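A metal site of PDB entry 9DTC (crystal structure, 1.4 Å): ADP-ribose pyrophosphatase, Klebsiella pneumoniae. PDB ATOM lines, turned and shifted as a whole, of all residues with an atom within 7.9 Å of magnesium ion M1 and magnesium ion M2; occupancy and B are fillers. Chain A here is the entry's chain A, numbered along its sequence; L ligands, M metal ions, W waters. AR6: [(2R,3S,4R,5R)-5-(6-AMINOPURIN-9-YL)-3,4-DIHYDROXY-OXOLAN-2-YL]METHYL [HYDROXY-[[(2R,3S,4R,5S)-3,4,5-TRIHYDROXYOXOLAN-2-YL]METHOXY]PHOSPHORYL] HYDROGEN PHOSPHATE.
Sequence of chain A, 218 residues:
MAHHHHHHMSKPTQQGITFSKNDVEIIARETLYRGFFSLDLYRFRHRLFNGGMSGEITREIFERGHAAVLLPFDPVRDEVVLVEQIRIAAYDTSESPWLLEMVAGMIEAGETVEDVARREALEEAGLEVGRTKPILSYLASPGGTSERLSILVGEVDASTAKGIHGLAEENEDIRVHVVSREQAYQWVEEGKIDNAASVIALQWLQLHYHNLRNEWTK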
ATOM      1  N   ALA A  68      18.845  10.790   2.865  1.00  0.00           N
ATOM      2  CA  ALA A  68      17.656  11.625   2.911  1.00  0.00           C
ATOM      3  C   ALA A  68      17.118  11.810   1.494  1.00  0.00           C
ATOM      4  O   ALA A  68      17.906  11.976   0.541  1.00  0.00           O
ATOM      5  CB  ALA A  68      18.000  12.986   3.510  1.00  0.00           C
ATOM      6  N   VAL A  83      14.429  14.733 -10.897  1.00  0.00           N
ATOM      7  CA  VAL A  83      15.809  14.911 -11.336  1.00  0.00           C
ATOM      8  C   VAL A  83      16.250  13.685 -12.129  1.00  0.00           C
ATOM      9  O   VAL A  83      15.941  12.542 -11.768  1.00  0.00           O
ATOM     10  CB  VAL A  83      16.793  15.228 -10.192  1.00  0.00           C
ATOM     11  CG1 VAL A  83      16.490  16.594  -9.641  1.00  0.00           C
ATOM     12  CG2 VAL A  83      16.758  14.199  -9.129  1.00  0.00           C
ATOM     13  N   GLN A  85      19.487  11.586 -13.828  1.00  0.00           N
ATOM     14  CA  GLN A  85      20.921  11.369 -13.854  1.00  0.00           C
ATOM     15  C   GLN A  85      21.185   9.899 -14.129  1.00  0.00           C
ATOM     16  O   GLN A  85      20.302   9.061 -13.980  1.00  0.00           O
ATOM     17  CB  GLN A  85      21.592  11.766 -12.531  1.00  0.00           C
ATOM     18  CG  GLN A  85      21.213  10.857 -11.375  1.00  0.00           C
ATOM     19  CD  GLN A  85      21.402  11.535 -10.035  1.00  0.00           C
ATOM     20  OE1 GLN A  85      22.527  11.848  -9.638  1.00  0.00           O
ATOM     21  NE2 GLN A  85      20.314  11.794  -9.340  1.00  0.00           N
ATOM     22  N   ARG A  87      22.554   6.256 -13.493  1.00  0.00           N
ATOM     23  CA  ARG A  87      22.765   5.307 -12.388  1.00  0.00           C
ATOM     24  C   ARG A  87      23.273   4.041 -13.070  1.00  0.00           C
ATOM     25  O   ARG A  87      22.497   3.237 -13.584  1.00  0.00           O
ATOM     26  CB  ARG A  87      21.474   5.058 -11.596  1.00  0.00           C
ATOM     27  CG  ARG A  87      20.914   6.281 -10.900  1.00  0.00           C
ATOM     28  CD  ARG A  87      21.836   6.781  -9.817  1.00  0.00           C
ATOM     29  NE  ARG A  87      21.189   7.812  -9.018  1.00  0.00           N
ATOM     30  CZ  ARG A  87      21.729   8.385  -7.962  1.00  0.00           C
ATOM     31  NH1 ARG A  87      22.991   8.184  -7.634  1.00  0.00           N
ATOM     32  NH2 ARG A  87      20.974   9.174  -7.193  1.00  0.00           N
ATOM     33  N   GLU A 101      14.199  10.569 -10.836  1.00  0.00           N
ATOM     34  CA  GLU A 101      14.306  10.297  -9.409  1.00  0.00           C
ATOM     35  C   GLU A 101      13.939  11.498  -8.553  1.00  0.00           C
ATOM     36  O   GLU A 101      13.716  12.610  -9.039  1.00  0.00           O
ATOM     37  CB  GLU A 101      15.750   9.938  -9.035  1.00  0.00           C
ATOM     38  CG  GLU A 101      16.319   8.732  -9.758  1.00  0.00           C
ATOM     39  CD  GLU A 101      17.739   8.428  -9.327  1.00  0.00           C
ATOM     40  OE1 GLU A 101      18.516   9.371  -9.076  1.00  0.00           O
ATOM     41  OE2 GLU A 101      18.071   7.227  -9.198  1.00  0.00           O
ATOM     42  N   MET A 102      13.872  11.237  -7.256  1.00  0.00           N
ATOM     43  CA  MET A 102      13.753  12.240  -6.215  1.00  0.00           C
ATOM     44  C   MET A 102      15.121  12.840  -5.901  1.00  0.00           C
ATOM     45  O   MET A 102      16.144  12.184  -6.025  1.00  0.00           O
ATOM     46  CB  MET A 102      13.240  11.602  -4.917  1.00  0.00           C
ATOM     47  CG  MET A 102      12.008  10.770  -5.059  1.00  0.00           C
ATOM     48  SD  MET A 102      10.532  11.732  -5.320  1.00  0.00           S
ATOM     49  CE  MET A 102      10.456  11.796  -7.103  1.00  0.00           C
ATOM     50  N   VAL A 103      15.104  14.098  -5.449  1.00  0.00           N
ATOM     51  CA  VAL A 103      16.278  14.677  -4.813  1.00  0.00           C
ATOM     52  C   VAL A 103      16.698  13.809  -3.656  1.00  0.00           C
ATOM     53  O   VAL A 103      15.858  13.329  -2.880  1.00  0.00           O
ATOM     54  CB  VAL A 103      15.911  16.097  -4.345  1.00  0.00           C
ATOM     55  CG1 VAL A 103      16.976  16.671  -3.429  1.00  0.00           C
ATOM     56  CG2 VAL A 103      15.626  17.000  -5.559  1.00  0.00           C
ATOM     57  N   ALA A 104      18.000  13.559  -3.526  1.00  0.00           N
ATOM     58  CA  ALA A 104      18.438  12.631  -2.483  1.00  0.00           C
ATOM     59  C   ALA A 104      19.940  12.749  -2.286  1.00  0.00           C
ATOM     60  O   ALA A 104      20.694  12.999  -3.238  1.00  0.00           O
ATOM     61  CB  ALA A 104      18.111  11.177  -2.836  1.00  0.00           C
ATOM     62  N   GLY A 105      20.380  12.491  -1.054  1.00  0.00           N
ATOM     63  CA  GLY A 105      21.810  12.450  -0.779  1.00  0.00           C
ATOM     64  C   GLY A 105      22.106  11.730   0.516  1.00  0.00           C
ATOM     65  O   GLY A 105      21.209  11.521   1.356  1.00  0.00           O
ATOM     66  N   MET A 106      23.380  11.393   0.688  1.00  0.00           N
ATOM     67  CA  MET A 106      23.797  10.700   1.890  1.00  0.00           C
ATOM     68  C   MET A 106      23.834  11.646   3.079  1.00  0.00           C
ATOM     69  O   MET A 106      24.096  12.846   2.944  1.00  0.00           O
ATOM     70  CB  MET A 106      25.192  10.106   1.692  1.00  0.00           C
ATOM     71  N   VAL A 116      19.861  17.725   5.132  1.00  0.00           N
ATOM     72  CA  VAL A 116      20.385  17.153   3.903  1.00  0.00           C
ATOM     73  C   VAL A 116      19.398  17.350   2.748  1.00  0.00           C
ATOM     74  O   VAL A 116      19.785  17.726   1.646  1.00  0.00           O
ATOM     75  CB  VAL A 116      20.747  15.667   4.106  1.00  0.00           C
ATOM     76  CG1 VAL A 116      21.106  15.018   2.765  1.00  0.00           C
ATOM     77  CG2 VAL A 116      21.886  15.538   5.116  1.00  0.00           C
ATOM     78  N   ARG A 119      19.579  20.933   1.479  1.00  0.00           N
ATOM     79  CA  ARG A 119      20.811  21.195   0.760  1.00  0.00           C
ATOM     80  C   ARG A 119      20.810  20.526  -0.597  1.00  0.00           C
ATOM     81  O   ARG A 119      21.194  21.135  -1.603  1.00  0.00           O
ATOM     82  CB  ARG A 119      22.008  20.749   1.595  1.00  0.00           C
ATOM     83  CG  ARG A 119      23.341  20.848   0.864  1.00  0.00           C
ATOM     84  CD  ARG A 119      24.521  20.510   1.767  1.00  0.00           C
ATOM     85  NE  ARG A 119      24.394  19.211   2.430  1.00  0.00           N
ATOM     86  CZ  ARG A 119      24.581  18.043   1.835  1.00  0.00           C
ATOM     87  NH1 ARG A 119      24.786  17.956   0.528  1.00  0.00           N
ATOM     88  NH2 ARG A 119      24.565  16.941   2.582  1.00  0.00           N
ATOM     89  N   GLU A 120      20.378  19.268  -0.667  1.00  0.00           N
ATOM     90  CA  GLU A 120      20.379  18.577  -1.939  1.00  0.00           C
ATOM     91  C   GLU A 120      19.361  19.166  -2.892  1.00  0.00           C
ATOM     92  O   GLU A 120      19.588  19.186  -4.106  1.00  0.00           O
ATOM     93  CB  GLU A 120      20.154  17.073  -1.751  1.00  0.00           C
ATOM     94  CG  GLU A 120      21.230  16.366  -0.941  1.00  0.00           C
ATOM     95  CD  GLU A 120      22.491  16.036  -1.736  1.00  0.00           C
ATOM     96  OE1 GLU A 120      22.490  16.175  -2.974  1.00  0.00           O
ATOM     97  OE2 GLU A 120      23.482  15.602  -1.112  1.00  0.00           O
ATOM     98  N   ALA A 121      18.241  19.696  -2.392  1.00  0.00           N
ATOM     99  CA  ALA A 121      17.271  20.291  -3.305  1.00  0.00           C
ATOM    100  C   ALA A 121      17.885  21.476  -4.032  1.00  0.00           C
ATOM    101  O   ALA A 121      17.635  21.686  -5.220  1.00  0.00           O
ATOM    102  CB  ALA A 121      16.019  20.720  -2.532  1.00  0.00           C
ATOM    103  N   GLU A 123      21.323  21.945  -4.495  1.00  0.00           N
ATOM    104  CA  GLU A 123      22.434  21.499  -5.319  1.00  0.00           C
ATOM    105  C   GLU A 123      21.966  20.735  -6.548  1.00  0.00           C
ATOM    106  O   GLU A 123      22.575  20.837  -7.621  1.00  0.00           O
ATOM    107  CB  GLU A 123      23.361  20.584  -4.511  1.00  0.00           C
ATOM    108  CG  GLU A 123      24.031  21.214  -3.311  1.00  0.00           C
ATOM    109  CD  GLU A 123      24.938  20.228  -2.588  1.00  0.00           C
ATOM    110  OE1 GLU A 123      24.937  19.018  -2.947  1.00  0.00           O
ATOM    111  OE2 GLU A 123      25.652  20.648  -1.650  1.00  0.00           O
ATOM    112  N   GLU A 124      20.918  19.924  -6.414  1.00  0.00           N
ATOM    113  CA  GLU A 124      20.529  19.022  -7.472  1.00  0.00           C
ATOM    114  C   GLU A 124      19.479  19.592  -8.408  1.00  0.00           C
ATOM    115  O   GLU A 124      19.399  19.146  -9.562  1.00  0.00           O
ATOM    116  CB  GLU A 124      20.045  17.693  -6.874  1.00  0.00           C
ATOM    117  CG  GLU A 124      21.105  16.987  -6.080  1.00  0.00           C
ATOM    118  CD  GLU A 124      20.797  15.516  -5.785  1.00  0.00           C
ATOM    119  OE1 GLU A 124      19.615  15.113  -5.886  1.00  0.00           O
ATOM    120  OE2 GLU A 124      21.740  14.770  -5.444  1.00  0.00           O
ATOM    121  N   GLY A 166      23.760  19.705 -10.243  1.00  0.00           N
ATOM    122  CA  GLY A 166      24.709  18.730  -9.771  1.00  0.00           C
ATOM    123  C   GLY A 166      26.090  19.336  -9.583  1.00  0.00           C
ATOM    124  O   GLY A 166      26.447  20.354 -10.180  1.00  0.00           O
ATOM    125  N   LEU A 167      26.881  18.667  -8.749  1.00  0.00           N
ATOM    126  CA  LEU A 167      28.251  19.092  -8.465  1.00  0.00           C
ATOM    127  C   LEU A 167      29.187  18.410  -9.467  1.00  0.00           C
ATOM    128  O   LEU A 167      29.434  17.204  -9.367  1.00  0.00           O
ATOM    129  CB  LEU A 167      28.636  18.732  -7.036  1.00  0.00           C
ATOM    130  CG  LEU A 167      27.604  19.122  -5.973  1.00  0.00           C
ATOM    131  CD1 LEU A 167      28.070  18.694  -4.597  1.00  0.00           C
ATOM    132  CD2 LEU A 167      27.326  20.626  -6.011  1.00  0.00           C
ATOM    133  N   GLU A 170      32.081  16.306  -8.354  1.00  0.00           N
ATOM    134  CA  GLU A 170      31.780  14.922  -8.012  1.00  0.00           C
ATOM    135  C   GLU A 170      31.249  14.131  -9.199  1.00  0.00           C
ATOM    136  O   GLU A 170      30.681  13.039  -9.003  1.00  0.00           O
ATOM    137  CB  GLU A 170      30.773  14.883  -6.861  1.00  0.00           C
ATOM    138  N   GLU A 172      28.675  14.656 -10.963  1.00  0.00           N
ATOM    139  CA  GLU A 172      27.238  14.558 -10.725  1.00  0.00           C
ATOM    140  C   GLU A 172      26.568  15.522 -11.690  1.00  0.00           C
ATOM    141  O   GLU A 172      26.638  16.736 -11.508  1.00  0.00           O
ATOM    142  CB  GLU A 172      26.936  14.939  -9.271  1.00  0.00           C
ATOM    143  CG  GLU A 172      25.503  14.693  -8.819  1.00  0.00           C
ATOM    144  CD  GLU A 172      25.175  15.408  -7.514  1.00  0.00           C
ATOM    145  OE1 GLU A 172      25.593  16.588  -7.350  1.00  0.00           O
ATOM    146  OE2 GLU A 172      24.519  14.796  -6.642  1.00  0.00           O
ATOM    147  N   ILE A 174      23.026  16.488 -13.520  1.00  0.00           N
ATOM    148  CA  ILE A 174      21.605  16.307 -13.207  1.00  0.00           C
ATOM    149  C   ILE A 174      20.771  17.266 -14.045  1.00  0.00           C
ATOM    150  O   ILE A 174      21.104  18.450 -14.145  1.00  0.00           O
ATOM    151  CB  ILE A 174      21.328  16.540 -11.707  1.00  0.00           C
ATOM    152  CG1 ILE A 174      22.161  15.556 -10.870  1.00  0.00           C
ATOM    153  CG2 ILE A 174      19.828  16.381 -11.400  1.00  0.00           C
ATOM    154  CD1 ILE A 174      22.056  15.683  -9.366  1.00  0.00           C
HETATM  155  N1  AR6 L   1      30.578   4.408  -5.957  1.00  0.00           N
HETATM  156  C2  AR6 L   1      31.455   5.386  -5.815  1.00  0.00           C
HETATM  157  N3  AR6 L   1      31.216   6.659  -5.576  1.00  0.00           N
HETATM  158  C4  AR6 L   1      29.903   6.892  -5.473  1.00  0.00           C
HETATM  159  C5  AR6 L   1      28.876   5.963  -5.585  1.00  0.00           C
HETATM  160  C6  AR6 L   1      29.260   4.649  -5.855  1.00  0.00           C
HETATM  161  N6  AR6 L   1      28.377   3.655  -5.998  1.00  0.00           N
HETATM  162  N7  AR6 L   1      27.659   6.559  -5.419  1.00  0.00           N
HETATM  163  C8  AR6 L   1      27.942   7.810  -5.194  1.00  0.00           C
HETATM  164  N9  AR6 L   1      29.288   8.066  -5.205  1.00  0.00           N
HETATM  165  PA  AR6 L   1      25.296  10.515  -5.768  1.00  0.00           P
HETATM  166  PB  AR6 L   1      23.130   9.836  -4.173  1.00  0.00           P
HETATM  167  C1' AR6 L   1      29.943   9.343  -5.013  1.00  0.00           C
HETATM  168  O1A AR6 L   1      24.683  11.864  -5.577  1.00  0.00           O
HETATM  169  O1B AR6 L   1      23.964  10.632  -3.219  1.00  0.00           O
HETATM  170  C1D AR6 L   1      20.633   6.571  -4.653  1.00  0.00           C
HETATM  171  O1D AR6 L   1      19.738   5.705  -5.254  1.00  0.00           O
HETATM  172  C2' AR6 L   1      30.013  10.145  -6.311  1.00  0.00           C
HETATM  173  O2' AR6 L   1      31.260  10.749  -6.428  1.00  0.00           O
HETATM  174  O2A AR6 L   1      25.881  10.166  -7.108  1.00  0.00           O
HETATM  175  O2B AR6 L   1      21.908  10.514  -4.807  1.00  0.00           O
HETATM  176  C2D AR6 L   1      21.602   5.729  -3.802  1.00  0.00           C
HETATM  177  O2D AR6 L   1      21.459   4.351  -4.134  1.00  0.00           O
HETATM  178  C3' AR6 L   1      28.845  11.121  -6.185  1.00  0.00           C
HETATM  179  O3' AR6 L   1      29.207  12.366  -6.728  1.00  0.00           O
HETATM  180  O3A AR6 L   1      24.261   9.341  -5.246  1.00  0.00           O
HETATM  181  C3D AR6 L   1      21.132   6.090  -2.379  1.00  0.00           C
HETATM  182  O3D AR6 L   1      20.164   5.273  -1.861  1.00  0.00           O
HETATM  183  C4' AR6 L   1      28.689  11.276  -4.670  1.00  0.00           C
HETATM  184  O4' AR6 L   1      29.240  10.108  -4.077  1.00  0.00           O
HETATM  185  C4D AR6 L   1      20.586   7.512  -2.533  1.00  0.00           C
HETATM  186  O4D AR6 L   1      19.956   7.490  -3.813  1.00  0.00           O
HETATM  187  C5' AR6 L   1      27.227  11.469  -4.257  1.00  0.00           C
HETATM  188  O5' AR6 L   1      26.433  10.340  -4.584  1.00  0.00           O
HETATM  189  C5D AR6 L   1      21.675   8.560  -2.424  1.00  0.00           C
HETATM  190  O5D AR6 L   1      22.625   8.424  -3.475  1.00  0.00           O
HETATM  191 MG    MG M   1      23.614  15.285  -4.644  1.00  0.00          MG
HETATM  192 MG    MG M   2      21.734  12.593  -5.198  1.00  0.00          MG
HETATM  193  O   HOH W   1      25.699  15.235  -4.042  1.00  0.00           O
HETATM  194  O   HOH W   2      23.033  12.533  -6.979  1.00  0.00           O
HETATM  195  O   HOH W   3      24.121  17.355  -5.110  1.00  0.00           O
HETATM  196  O   HOH W   4      19.890  12.549  -6.449  1.00  0.00           O
HETATM  197  O   HOH W   5      23.460  13.232  -3.964  1.00  0.00           O
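Of the 21 residues printed, 3 come within 4 Å of magnesium ion M2.
Magnesium ion M1 is bound by OE2 of Glu 124 (2.1 Å), water W5 (2.2 Å), water W1 (2.2 Å), water W3 (2.2 Å), OE1 of Glu 120 (2.2 Å) and OE2 of Glu 172 (2.2 Å). Magnesium ion M1 has six donor atoms within binding distance.
Magnesium ion M2 is bound by an oxygen (O2B) of the ligand, the side-chain carboxylate (OE2) of Glu 124, water W2, water W5, water W4 and the backbone carbonyl oxygen (O) of Ala 104.
Water W3 lies within hydrogen-bond range of the side-chain carboxylate of Glu 172 (2.8 Å) and the side-chain carboxylate of Glu 123 (2.8 Å). Water W4 bridges OE1 of Glu 124 (2.6 Å) and NE2 of Gln 85 (3.0 Å).
Within 4 Å of magnesium ion M1: Ala 104, Glu 120, Glu 124 and Glu 172.
O of Glu 170 is in hydrogen-bond range of O3' of the ligand (2.8 Å). The guanidinium group (NH1) of Arg 87 is in salt-bridge range of an oxygen (O2A) of the ligand (3.5 Å).
N of Leu 167 sits at hydrogen-bond distance from OE1 of Glu 172 (2.8 Å). OE2 of Glu 120 is in salt-bridge range of NH1 of Arg 119 (3.2 Å).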
